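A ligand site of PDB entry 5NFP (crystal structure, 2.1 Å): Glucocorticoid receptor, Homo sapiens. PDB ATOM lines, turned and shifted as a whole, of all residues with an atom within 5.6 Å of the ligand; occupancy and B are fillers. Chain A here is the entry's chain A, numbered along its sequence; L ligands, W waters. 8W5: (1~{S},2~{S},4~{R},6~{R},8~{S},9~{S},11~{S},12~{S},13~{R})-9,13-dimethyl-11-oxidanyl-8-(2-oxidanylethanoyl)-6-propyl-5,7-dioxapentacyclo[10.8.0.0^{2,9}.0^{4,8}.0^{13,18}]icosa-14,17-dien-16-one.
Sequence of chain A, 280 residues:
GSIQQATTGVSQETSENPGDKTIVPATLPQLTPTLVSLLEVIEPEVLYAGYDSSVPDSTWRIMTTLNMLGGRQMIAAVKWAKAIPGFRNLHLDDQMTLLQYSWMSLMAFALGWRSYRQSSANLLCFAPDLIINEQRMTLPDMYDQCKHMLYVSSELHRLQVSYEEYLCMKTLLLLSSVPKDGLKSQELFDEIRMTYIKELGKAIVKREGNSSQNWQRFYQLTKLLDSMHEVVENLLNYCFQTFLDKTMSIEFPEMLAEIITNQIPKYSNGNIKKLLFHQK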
ATOM      1  N   ILE A  62      -9.972  10.858 -28.025  1.00  0.00           N
ATOM      2  CA  ILE A  62      -8.876   9.920 -28.308  1.00  0.00           C
ATOM      3  C   ILE A  62      -9.421   8.500 -28.551  1.00  0.00           C
ATOM      4  O   ILE A  62      -9.058   7.865 -29.537  1.00  0.00           O
ATOM      5  CB  ILE A  62      -7.755   9.981 -27.218  1.00  0.00           C
ATOM      6  CG1 ILE A  62      -7.000  11.336 -27.313  1.00  0.00           C
ATOM      7  CG2 ILE A  62      -6.762   8.783 -27.333  1.00  0.00           C
ATOM      8  CD1 ILE A  62      -6.125  11.683 -26.110  1.00  0.00           C
ATOM      9  N   MET A  63     -10.348   8.039 -27.688  1.00  0.00           N
ATOM     10  CA  MET A  63     -10.965   6.694 -27.828  1.00  0.00           C
ATOM     11  C   MET A  63     -11.710   6.562 -29.151  1.00  0.00           C
ATOM     12  O   MET A  63     -11.586   5.540 -29.827  1.00  0.00           O
ATOM     13  CB  MET A  63     -11.901   6.399 -26.657  1.00  0.00           C
ATOM     14  CG  MET A  63     -11.172   6.181 -25.345  1.00  0.00           C
ATOM     15  SD  MET A  63     -12.283   6.072 -23.923  1.00  0.00           S
ATOM     16  CE  MET A  63     -12.880   4.476 -24.115  1.00  0.00           C
ATOM     17  N   LEU A  66      -9.271   6.512 -32.097  1.00  0.00           N
ATOM     18  CA  LEU A  66      -8.598   5.201 -32.101  1.00  0.00           C
ATOM     19  C   LEU A  66      -9.482   4.087 -32.636  1.00  0.00           C
ATOM     20  O   LEU A  66      -8.966   3.195 -33.293  1.00  0.00           O
ATOM     21  CB  LEU A  66      -7.997   4.847 -30.730  1.00  0.00           C
ATOM     22  CG  LEU A  66      -6.846   5.729 -30.230  1.00  0.00           C
ATOM     23  CD1 LEU A  66      -6.425   5.332 -28.830  1.00  0.00           C
ATOM     24  CD2 LEU A  66      -5.643   5.686 -31.169  1.00  0.00           C
ATOM     25  N   ASN A  67     -10.811   4.132 -32.382  1.00  0.00           N
ATOM     26  CA  ASN A  67     -11.707   3.104 -32.926  1.00  0.00           C
ATOM     27  C   ASN A  67     -11.737   3.189 -34.448  1.00  0.00           C
ATOM     28  O   ASN A  67     -11.648   2.161 -35.098  1.00  0.00           O
ATOM     29  CB  ASN A  67     -13.120   3.185 -32.332  1.00  0.00           C
ATOM     30  CG  ASN A  67     -13.162   2.721 -30.895  1.00  0.00           C
ATOM     31  OD1 ASN A  67     -12.351   1.902 -30.458  1.00  0.00           O
ATOM     32  ND2 ASN A  67     -14.141   3.190 -30.132  1.00  0.00           N
ATOM     33  N   LEU A  69      -9.293   4.460 -36.382  1.00  0.00           N
ATOM     34  CA  LEU A  69      -7.965   3.984 -36.767  1.00  0.00           C
ATOM     35  C   LEU A  69      -7.921   2.450 -36.738  1.00  0.00           C
ATOM     36  O   LEU A  69      -7.416   1.840 -37.685  1.00  0.00           O
ATOM     37  CB  LEU A  69      -6.876   4.604 -35.857  1.00  0.00           C
ATOM     38  CG  LEU A  69      -5.419   4.108 -36.084  1.00  0.00           C
ATOM     39  CD1 LEU A  69      -4.892   4.475 -37.517  1.00  0.00           C
ATOM     40  CD2 LEU A  69      -4.507   4.645 -34.988  1.00  0.00           C
ATOM     41  N   GLY A  70      -8.479   1.861 -35.678  1.00  0.00           N
ATOM     42  CA  GLY A  70      -8.566   0.422 -35.507  1.00  0.00           C
ATOM     43  C   GLY A  70      -9.297  -0.283 -36.646  1.00  0.00           C
ATOM     44  O   GLY A  70      -8.884  -1.349 -37.071  1.00  0.00           O
ATOM     45  N   GLN A  73      -6.968  -0.255 -39.583  1.00  0.00           N
ATOM     46  CA  GLN A  73      -5.886  -1.220 -39.335  1.00  0.00           C
ATOM     47  C   GLN A  73      -6.398  -2.646 -39.499  1.00  0.00           C
ATOM     48  O   GLN A  73      -5.661  -3.502 -39.982  1.00  0.00           O
ATOM     49  CB  GLN A  73      -5.305  -1.057 -37.915  1.00  0.00           C
ATOM     50  CG  GLN A  73      -4.395   0.173 -37.759  1.00  0.00           C
ATOM     51  CD  GLN A  73      -3.930   0.363 -36.320  1.00  0.00           C
ATOM     52  OE1 GLN A  73      -3.242   1.320 -35.995  1.00  0.00           O
ATOM     53  NE2 GLN A  73      -4.239  -0.580 -35.455  1.00  0.00           N
ATOM     54  N   TRP A 103      -8.091 -10.444 -33.510  1.00  0.00           N
ATOM     55  CA  TRP A 103      -7.998  -9.024 -33.918  1.00  0.00           C
ATOM     56  C   TRP A 103      -7.352  -8.116 -32.842  1.00  0.00           C
ATOM     57  O   TRP A 103      -6.410  -7.400 -33.171  1.00  0.00           O
ATOM     58  CB  TRP A 103      -9.368  -8.477 -34.382  1.00  0.00           C
ATOM     59  CG  TRP A 103     -10.304  -8.090 -33.274  1.00  0.00           C
ATOM     60  CD1 TRP A 103     -11.089  -8.922 -32.539  1.00  0.00           C
ATOM     61  CD2 TRP A 103     -10.506  -6.773 -32.747  1.00  0.00           C
ATOM     62  NE1 TRP A 103     -11.763  -8.196 -31.576  1.00  0.00           N
ATOM     63  CE2 TRP A 103     -11.479  -6.864 -31.732  1.00  0.00           C
ATOM     64  CE3 TRP A 103      -9.942  -5.510 -33.028  1.00  0.00           C
ATOM     65  CZ2 TRP A 103     -11.940  -5.749 -31.020  1.00  0.00           C
ATOM     66  CZ3 TRP A 103     -10.374  -4.406 -32.304  1.00  0.00           C
ATOM     67  CH2 TRP A 103     -11.369  -4.535 -31.320  1.00  0.00           C
ATOM     68  N   MET A 104      -7.830  -8.173 -31.581  1.00  0.00           N
ATOM     69  CA  MET A 104      -7.305  -7.326 -30.515  1.00  0.00           C
ATOM     70  C   MET A 104      -5.828  -7.664 -30.187  1.00  0.00           C
ATOM     71  O   MET A 104      -5.034  -6.745 -29.963  1.00  0.00           O
ATOM     72  CB  MET A 104      -8.187  -7.423 -29.244  1.00  0.00           C
ATOM     73  CG  MET A 104      -7.728  -6.459 -28.109  1.00  0.00           C
ATOM     74  SD  MET A 104      -7.847  -4.712 -28.612  1.00  0.00           S
ATOM     75  CE  MET A 104      -9.584  -4.403 -28.248  1.00  0.00           C
ATOM     76  N   MET A 107      -3.658  -6.130 -32.974  1.00  0.00           N
ATOM     77  CA  MET A 107      -3.591  -4.670 -32.828  1.00  0.00           C
ATOM     78  C   MET A 107      -2.697  -4.256 -31.696  1.00  0.00           C
ATOM     79  O   MET A 107      -1.892  -3.354 -31.875  1.00  0.00           O
ATOM     80  CB  MET A 107      -4.966  -4.030 -32.659  1.00  0.00           C
ATOM     81  CG  MET A 107      -5.953  -4.350 -33.749  1.00  0.00           C
ATOM     82  SD  MET A 107      -5.569  -3.513 -35.293  1.00  0.00           S
ATOM     83  CE  MET A 107      -4.620  -4.747 -36.122  1.00  0.00           C
ATOM     84  N   ALA A 108      -2.859  -4.897 -30.507  1.00  0.00           N
ATOM     85  CA  ALA A 108      -2.059  -4.551 -29.336  1.00  0.00           C
ATOM     86  C   ALA A 108      -0.586  -4.931 -29.520  1.00  0.00           C
ATOM     87  O   ALA A 108       0.300  -4.211 -29.021  1.00  0.00           O
ATOM     88  CB  ALA A 108      -2.632  -5.226 -28.093  1.00  0.00           C
ATOM     89  N   LEU A 111       0.978  -2.455 -31.981  1.00  0.00           N
ATOM     90  CA  LEU A 111       1.100  -1.190 -31.226  1.00  0.00           C
ATOM     91  C   LEU A 111       2.306  -1.240 -30.284  1.00  0.00           C
ATOM     92  O   LEU A 111       3.057  -0.263 -30.163  1.00  0.00           O
ATOM     93  CB  LEU A 111      -0.192  -0.923 -30.424  1.00  0.00           C
ATOM     94  CG  LEU A 111      -0.109   0.109 -29.289  1.00  0.00           C
ATOM     95  CD1 LEU A 111       0.074   1.518 -29.807  1.00  0.00           C
ATOM     96  CD2 LEU A 111      -1.326   0.022 -28.439  1.00  0.00           C
ATOM     97  N   ARG A 114       5.450  -0.738 -32.455  1.00  0.00           N
ATOM     98  CA  ARG A 114       5.613   0.672 -32.871  1.00  0.00           C
ATOM     99  C   ARG A 114       6.072   1.527 -31.704  1.00  0.00           C
ATOM    100  O   ARG A 114       6.906   2.414 -31.908  1.00  0.00           O
ATOM    101  CB  ARG A 114       4.310   1.265 -33.454  1.00  0.00           C
ATOM    102  CG  ARG A 114       3.872   0.660 -34.772  1.00  0.00           C
ATOM    103  CD  ARG A 114       2.727   1.426 -35.441  1.00  0.00           C
ATOM    104  NE  ARG A 114       1.515   1.605 -34.614  1.00  0.00           N
ATOM    105  CZ  ARG A 114       0.527   0.727 -34.507  1.00  0.00           C
ATOM    106  NH1 ARG A 114       0.603  -0.459 -35.093  1.00  0.00           N
ATOM    107  NH2 ARG A 114      -0.544   1.017 -33.774  1.00  0.00           N
ATOM    108  N   PHE A 126       0.239   4.903 -31.171  1.00  0.00           N
ATOM    109  CA  PHE A 126      -0.913   4.392 -31.940  1.00  0.00           C
ATOM    110  C   PHE A 126      -0.742   4.711 -33.415  1.00  0.00           C
ATOM    111  O   PHE A 126      -0.937   3.838 -34.268  1.00  0.00           O
ATOM    112  CB  PHE A 126      -2.222   4.962 -31.386  1.00  0.00           C
ATOM    113  CG  PHE A 126      -2.658   4.326 -30.087  1.00  0.00           C
ATOM    114  CD1 PHE A 126      -3.343   3.116 -30.073  1.00  0.00           C
ATOM    115  CD2 PHE A 126      -2.437   4.975 -28.873  1.00  0.00           C
ATOM    116  CE1 PHE A 126      -3.771   2.548 -28.866  1.00  0.00           C
ATOM    117  CE2 PHE A 126      -2.866   4.407 -27.666  1.00  0.00           C
ATOM    118  CZ  PHE A 126      -3.498   3.177 -27.670  1.00  0.00           C
ATOM    119  N   ILE A 132       0.500   8.705 -27.175  1.00  0.00           N
ATOM    120  CA  ILE A 132       0.025   8.950 -25.821  1.00  0.00           C
ATOM    121  C   ILE A 132       1.255   9.189 -24.947  1.00  0.00           C
ATOM    122  O   ILE A 132       1.947   8.241 -24.552  1.00  0.00           O
ATOM    123  CB  ILE A 132      -0.940   7.859 -25.240  1.00  0.00           C
ATOM    124  CG1 ILE A 132      -2.174   7.607 -26.152  1.00  0.00           C
ATOM    125  CG2 ILE A 132      -1.354   8.171 -23.780  1.00  0.00           C
ATOM    126  CD1 ILE A 132      -2.996   8.830 -26.667  1.00  0.00           C
ATOM    127  N   MET A 142      -7.191   7.491 -18.636  1.00  0.00           N
ATOM    128  CA  MET A 142      -6.256   7.145 -19.705  1.00  0.00           C
ATOM    129  C   MET A 142      -5.328   6.009 -19.290  1.00  0.00           C
ATOM    130  O   MET A 142      -5.232   5.016 -19.997  1.00  0.00           O
ATOM    131  CB  MET A 142      -5.405   8.355 -20.137  1.00  0.00           C
ATOM    132  CG  MET A 142      -5.864   8.986 -21.416  1.00  0.00           C
ATOM    133  SD  MET A 142      -5.760   7.947 -22.897  1.00  0.00           S
ATOM    134  CE  MET A 142      -7.333   8.224 -23.504  1.00  0.00           C
ATOM    135  N   GLN A 145      -6.476   2.129 -18.935  1.00  0.00           N
ATOM    136  CA  GLN A 145      -6.678   1.473 -20.223  1.00  0.00           C
ATOM    137  C   GLN A 145      -5.292   1.196 -20.858  1.00  0.00           C
ATOM    138  O   GLN A 145      -5.017   0.082 -21.298  1.00  0.00           O
ATOM    139  CB  GLN A 145      -7.563   2.345 -21.151  1.00  0.00           C
ATOM    140  CG  GLN A 145      -8.909   2.756 -20.512  1.00  0.00           C
ATOM    141  CD  GLN A 145      -9.782   3.569 -21.439  1.00  0.00           C
ATOM    142  OE1 GLN A 145     -10.551   3.027 -22.227  1.00  0.00           O
ATOM    143  NE2 GLN A 145      -9.731   4.885 -21.327  1.00  0.00           N
ATOM    144  N   CYS A 146      -4.400   2.203 -20.806  1.00  0.00           N
ATOM    145  CA  CYS A 146      -3.074   2.186 -21.409  1.00  0.00           C
ATOM    146  C   CYS A 146      -2.043   1.244 -20.764  1.00  0.00           C
ATOM    147  O   CYS A 146      -1.168   0.766 -21.489  1.00  0.00           O
ATOM    148  CB  CYS A 146      -2.532   3.607 -21.508  1.00  0.00           C
ATOM    149  SG  CYS A 146      -3.387   4.624 -22.742  1.00  0.00           S
ATOM    150  N   MET A 149      -1.440  -2.140 -22.479  1.00  0.00           N
ATOM    151  CA  MET A 149      -0.749  -1.967 -23.765  1.00  0.00           C
ATOM    152  C   MET A 149       0.712  -1.582 -23.564  1.00  0.00           C
ATOM    153  O   MET A 149       1.576  -2.073 -24.306  1.00  0.00           O
ATOM    154  CB  MET A 149      -1.509  -0.971 -24.645  1.00  0.00           C
ATOM    155  CG  MET A 149      -2.828  -1.529 -25.153  1.00  0.00           C
ATOM    156  SD  MET A 149      -3.831  -0.320 -26.039  1.00  0.00           S
ATOM    157  CE  MET A 149      -4.521   0.616 -24.670  1.00  0.00           C
ATOM    158  N   LEU A 235      -8.219  -5.607 -22.414  1.00  0.00           N
ATOM    159  CA  LEU A 235      -8.586  -4.668 -23.479  1.00  0.00           C
ATOM    160  C   LEU A 235     -10.017  -4.885 -23.982  1.00  0.00           C
ATOM    161  O   LEU A 235     -10.735  -3.916 -24.234  1.00  0.00           O
ATOM    162  CB  LEU A 235      -7.592  -4.718 -24.644  1.00  0.00           C
ATOM    163  CG  LEU A 235      -6.129  -4.358 -24.303  1.00  0.00           C
ATOM    164  CD1 LEU A 235      -5.271  -4.392 -25.540  1.00  0.00           C
ATOM    165  CD2 LEU A 235      -6.030  -3.006 -23.579  1.00  0.00           C
ATOM    166  N   TYR A 238     -12.829  -3.328 -21.704  1.00  0.00           N
ATOM    167  CA  TYR A 238     -13.084  -1.919 -22.029  1.00  0.00           C
ATOM    168  C   TYR A 238     -13.795  -1.793 -23.377  1.00  0.00           C
ATOM    169  O   TYR A 238     -14.763  -1.049 -23.522  1.00  0.00           O
ATOM    170  CB  TYR A 238     -11.791  -1.085 -22.081  1.00  0.00           C
ATOM    171  CG  TYR A 238     -11.110  -0.883 -20.751  1.00  0.00           C
ATOM    172  CD1 TYR A 238     -11.751  -0.201 -19.710  1.00  0.00           C
ATOM    173  CD2 TYR A 238      -9.786  -1.280 -20.550  1.00  0.00           C
ATOM    174  CE1 TYR A 238     -11.108   0.019 -18.493  1.00  0.00           C
ATOM    175  CE2 TYR A 238      -9.143  -1.074 -19.329  1.00  0.00           C
ATOM    176  CZ  TYR A 238      -9.800  -0.412 -18.308  1.00  0.00           C
ATOM    177  OH  TYR A 238      -9.197  -0.201 -17.094  1.00  0.00           O
ATOM    178  N   CYS A 239     -13.299  -2.534 -24.370  1.00  0.00           N
ATOM    179  CA  CYS A 239     -13.847  -2.536 -25.722  1.00  0.00           C
ATOM    180  C   CYS A 239     -15.342  -2.922 -25.728  1.00  0.00           C
ATOM    181  O   CYS A 239     -16.161  -2.192 -26.287  1.00  0.00           O
ATOM    182  CB  CYS A 239     -13.024  -3.432 -26.635  1.00  0.00           C
ATOM    183  SG  CYS A 239     -13.610  -3.443 -28.339  1.00  0.00           S
ATOM    184  N   THR A 242     -17.553  -0.245 -23.816  1.00  0.00           N
ATOM    185  CA  THR A 242     -17.762   0.995 -24.587  1.00  0.00           C
ATOM    186  C   THR A 242     -18.583   0.749 -25.844  1.00  0.00           C
ATOM    187  O   THR A 242     -19.243   1.672 -26.325  1.00  0.00           O
ATOM    188  CB  THR A 242     -16.434   1.707 -24.850  1.00  0.00           C
ATOM    189  OG1 THR A 242     -15.593   0.840 -25.587  1.00  0.00           O
ATOM    190  CG2 THR A 242     -15.730   2.153 -23.562  1.00  0.00           C
ATOM    191  N   ILE A 250     -19.721   6.210 -27.743  1.00  0.00           N
ATOM    192  CA  ILE A 250     -18.424   5.797 -28.288  1.00  0.00           C
ATOM    193  C   ILE A 250     -18.689   4.979 -29.551  1.00  0.00           C
ATOM    194  O   ILE A 250     -19.259   3.881 -29.507  1.00  0.00           O
ATOM    195  CB  ILE A 250     -17.485   5.142 -27.228  1.00  0.00           C
ATOM    196  CG1 ILE A 250     -17.012   6.209 -26.191  1.00  0.00           C
ATOM    197  CG2 ILE A 250     -16.282   4.478 -27.901  1.00  0.00           C
ATOM    198  CD1 ILE A 250     -16.344   5.693 -24.967  1.00  0.00           C
ATOM    199  N   PHE A 252     -17.865   2.942 -33.077  1.00  0.00           N
ATOM    200  CA  PHE A 252     -16.952   1.981 -33.639  1.00  0.00           C
ATOM    201  C   PHE A 252     -17.289   1.903 -35.142  1.00  0.00           C
ATOM    202  O   PHE A 252     -18.481   1.855 -35.496  1.00  0.00           O
ATOM    203  CB  PHE A 252     -17.121   0.590 -32.986  1.00  0.00           C
ATOM    204  CG  PHE A 252     -16.516   0.457 -31.613  1.00  0.00           C
ATOM    205  CD1 PHE A 252     -17.187   0.924 -30.479  1.00  0.00           C
ATOM    206  CD2 PHE A 252     -15.271  -0.153 -31.436  1.00  0.00           C
ATOM    207  CE1 PHE A 252     -16.625   0.799 -29.208  1.00  0.00           C
ATOM    208  CE2 PHE A 252     -14.738  -0.321 -30.161  1.00  0.00           C
ATOM    209  CZ  PHE A 252     -15.409   0.166 -29.059  1.00  0.00           C
ATOM    210  N   LEU A 256     -14.974  -2.918 -37.017  1.00  0.00           N
ATOM    211  CA  LEU A 256     -14.871  -3.289 -35.612  1.00  0.00           C
ATOM    212  C   LEU A 256     -16.225  -3.676 -35.026  1.00  0.00           C
ATOM    213  O   LEU A 256     -16.299  -4.683 -34.323  1.00  0.00           O
ATOM    214  CB  LEU A 256     -14.197  -2.165 -34.775  1.00  0.00           C
ATOM    215  CG  LEU A 256     -12.739  -1.836 -35.132  1.00  0.00           C
ATOM    216  CD1 LEU A 256     -12.038  -1.075 -33.981  1.00  0.00           C
ATOM    217  CD2 LEU A 256     -11.924  -3.126 -35.463  1.00  0.00           C
HETATM  218  C1  8W5 L   1      -6.184   5.101 -25.171  1.00  0.00           C
HETATM  219  C2  8W5 L   1      -7.598   4.511 -25.143  1.00  0.00           C
HETATM  220  C3  8W5 L   1      -7.463   2.996 -25.050  1.00  0.00           C
HETATM  221  C7  8W5 L   1      -9.464   0.097 -25.551  1.00  0.00           C
HETATM  222  C9  8W5 L   1      -8.590  -0.890 -26.397  1.00  0.00           C
HETATM  223  C10 8W5 L   1      -8.357  -0.083 -27.697  1.00  0.00           C
HETATM  224  C12 8W5 L   1      -7.728  -0.730 -28.940  1.00  0.00           C
HETATM  225  C14 8W5 L   1      -6.338  -1.316 -28.579  1.00  0.00           C
HETATM  226  C15 8W5 L   1      -5.571  -1.874 -29.820  1.00  0.00           C
HETATM  227  C16 8W5 L   1      -5.574  -0.809 -30.926  1.00  0.00           C
HETATM  228  C20 8W5 L   1      -5.613   1.228 -32.979  1.00  0.00           C
HETATM  229  C21 8W5 L   1      -6.764   0.864 -32.411  1.00  0.00           C
HETATM  230  C22 8W5 L   1      -6.899  -0.191 -31.350  1.00  0.00           C
HETATM  231  C27 8W5 L   1      -9.575   1.655 -29.015  1.00  0.00           C
HETATM  232  C31 8W5 L   1     -11.658   1.309 -26.351  1.00  0.00           C
HETATM  233  C33 8W5 L   1     -12.284   2.581 -26.870  1.00  0.00           C
HETATM  234  C35 8W5 L   1     -10.837  -0.501 -28.448  1.00  0.00           C
HETATM  235  C4  8W5 L   1      -8.820   2.283 -24.993  1.00  0.00           C
HETATM  236  O6  8W5 L   1      -8.562   0.882 -24.760  1.00  0.00           O
HETATM  237  C17 8W5 L   1      -4.417  -0.441 -31.478  1.00  0.00           C
HETATM  238  C18 8W5 L   1      -4.358   0.593 -32.539  1.00  0.00           C
HETATM  239  O19 8W5 L   1      -3.295   0.940 -33.040  1.00  0.00           O
HETATM  240  C23 8W5 L   1      -7.546   0.378 -30.046  1.00  0.00           C
HETATM  241  C25 8W5 L   1      -8.864   1.190 -30.315  1.00  0.00           C
HETATM  242  C28 8W5 L   1      -9.778   0.552 -27.967  1.00  0.00           C
HETATM  243  C29 8W5 L   1     -10.151   1.096 -26.545  1.00  0.00           C
HETATM  244  O30 8W5 L   1      -9.474   2.342 -26.289  1.00  0.00           O
HETATM  245  O32 8W5 L   1     -12.363   0.493 -25.806  1.00  0.00           O
HETATM  246  O34 8W5 L   1     -13.696   2.449 -26.967  1.00  0.00           O
HETATM  247  O36 8W5 L   1      -9.817   0.500 -31.136  1.00  0.00           O
HETATM  248  C37 8W5 L   1      -7.727  -1.320 -32.033  1.00  0.00           C
HETATM  249  O   HOH W   1      -1.990  -1.661 -34.092  1.00  0.00           O
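OG1 of Thr 242 lies within hydrogen-bond range of O34 of the ligand (2.8 Å).
NH2 of Arg 114 is in hydrogen-bond range of O19 of the ligand (2.8 Å).
O36 of the ligand lies within hydrogen-bond range of OD1 of Asn 67 (3.0 Å).
OE1 of Gln 73 sits close to O19 of the ligand, 3.0 Å away.
N of Cys 239 sits close to O32 of the ligand (3.5 Å).
The backbone carbonyl oxygen of Cys 239 is in hydrogen-bond range of the side-chain hydroxyl of Thr 242, 3.2 Å away.
The backbone carbonyl oxygen (O) of Tyr 238 sits at hydrogen-bond distance from the side-chain hydroxyl (OG1) of Thr 242.
NH2 of Arg 114 lies within hydrogen-bond range of O of Phe 126 (2.9 Å).
The side-chain amide nitrogen of Asn 67 sits close to the backbone carbonyl oxygen of Met 63.
NE2 of Gln 73 is in hydrogen-bond range of SD of Met 107, 3.2 Å away.
SG of Cys 146 lies within hydrogen-bond range of O of Met 142.
Met 63 touches the ligand.
O of Leu 66 touches C21 of the ligand, 3.3 Å away.
Gly 70 touches the ligand.
SD of Met 104 touches C14 of the ligand (3.7 Å).
Met 107 touches the ligand.
Phe 126 touches the ligand (CD1 to C18, 3.7 Å).
Met 142 touches the ligand (SD to C1, 3.7 Å).
OE1 of Gln 145 touches C4 of the ligand (3.3 Å).
Cys 146 touches the ligand.
SD of Met 149 touches C14 of the ligand (3.7 Å).
Tyr 238 touches the ligand.
Ile 250 touches the ligand.
Phe 252 touches the ligand.
Leu 256 touches the ligand (CD1 to O36, 3.9 Å).
Hydrophobic or aromatic side chains that line the ligand: Met 63, Leu 66, Met 104, Met 107, Phe 126, Met 142, Met 149, Ile 250, Phe 252 and Leu 256.
Within 4 Å of the ligand: Met 63, Leu 66, Asn 67, Gly 70, Gln 73, Met 104, Met 107, Arg 114, Phe 126, Met 142, Gln 145, Cys 146, Met 149, Tyr 238, Cys 239, Thr 242, Ile 250, Phe 252 and Leu 256.
The nearest printed residue that does not touch the ligand is Trp 103 (4.1 Å).
Water W1 lies within hydrogen-bond range of O of Met 107, NE2 of Gln 73, NH1 of Arg 114 and O19 of the ligand.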
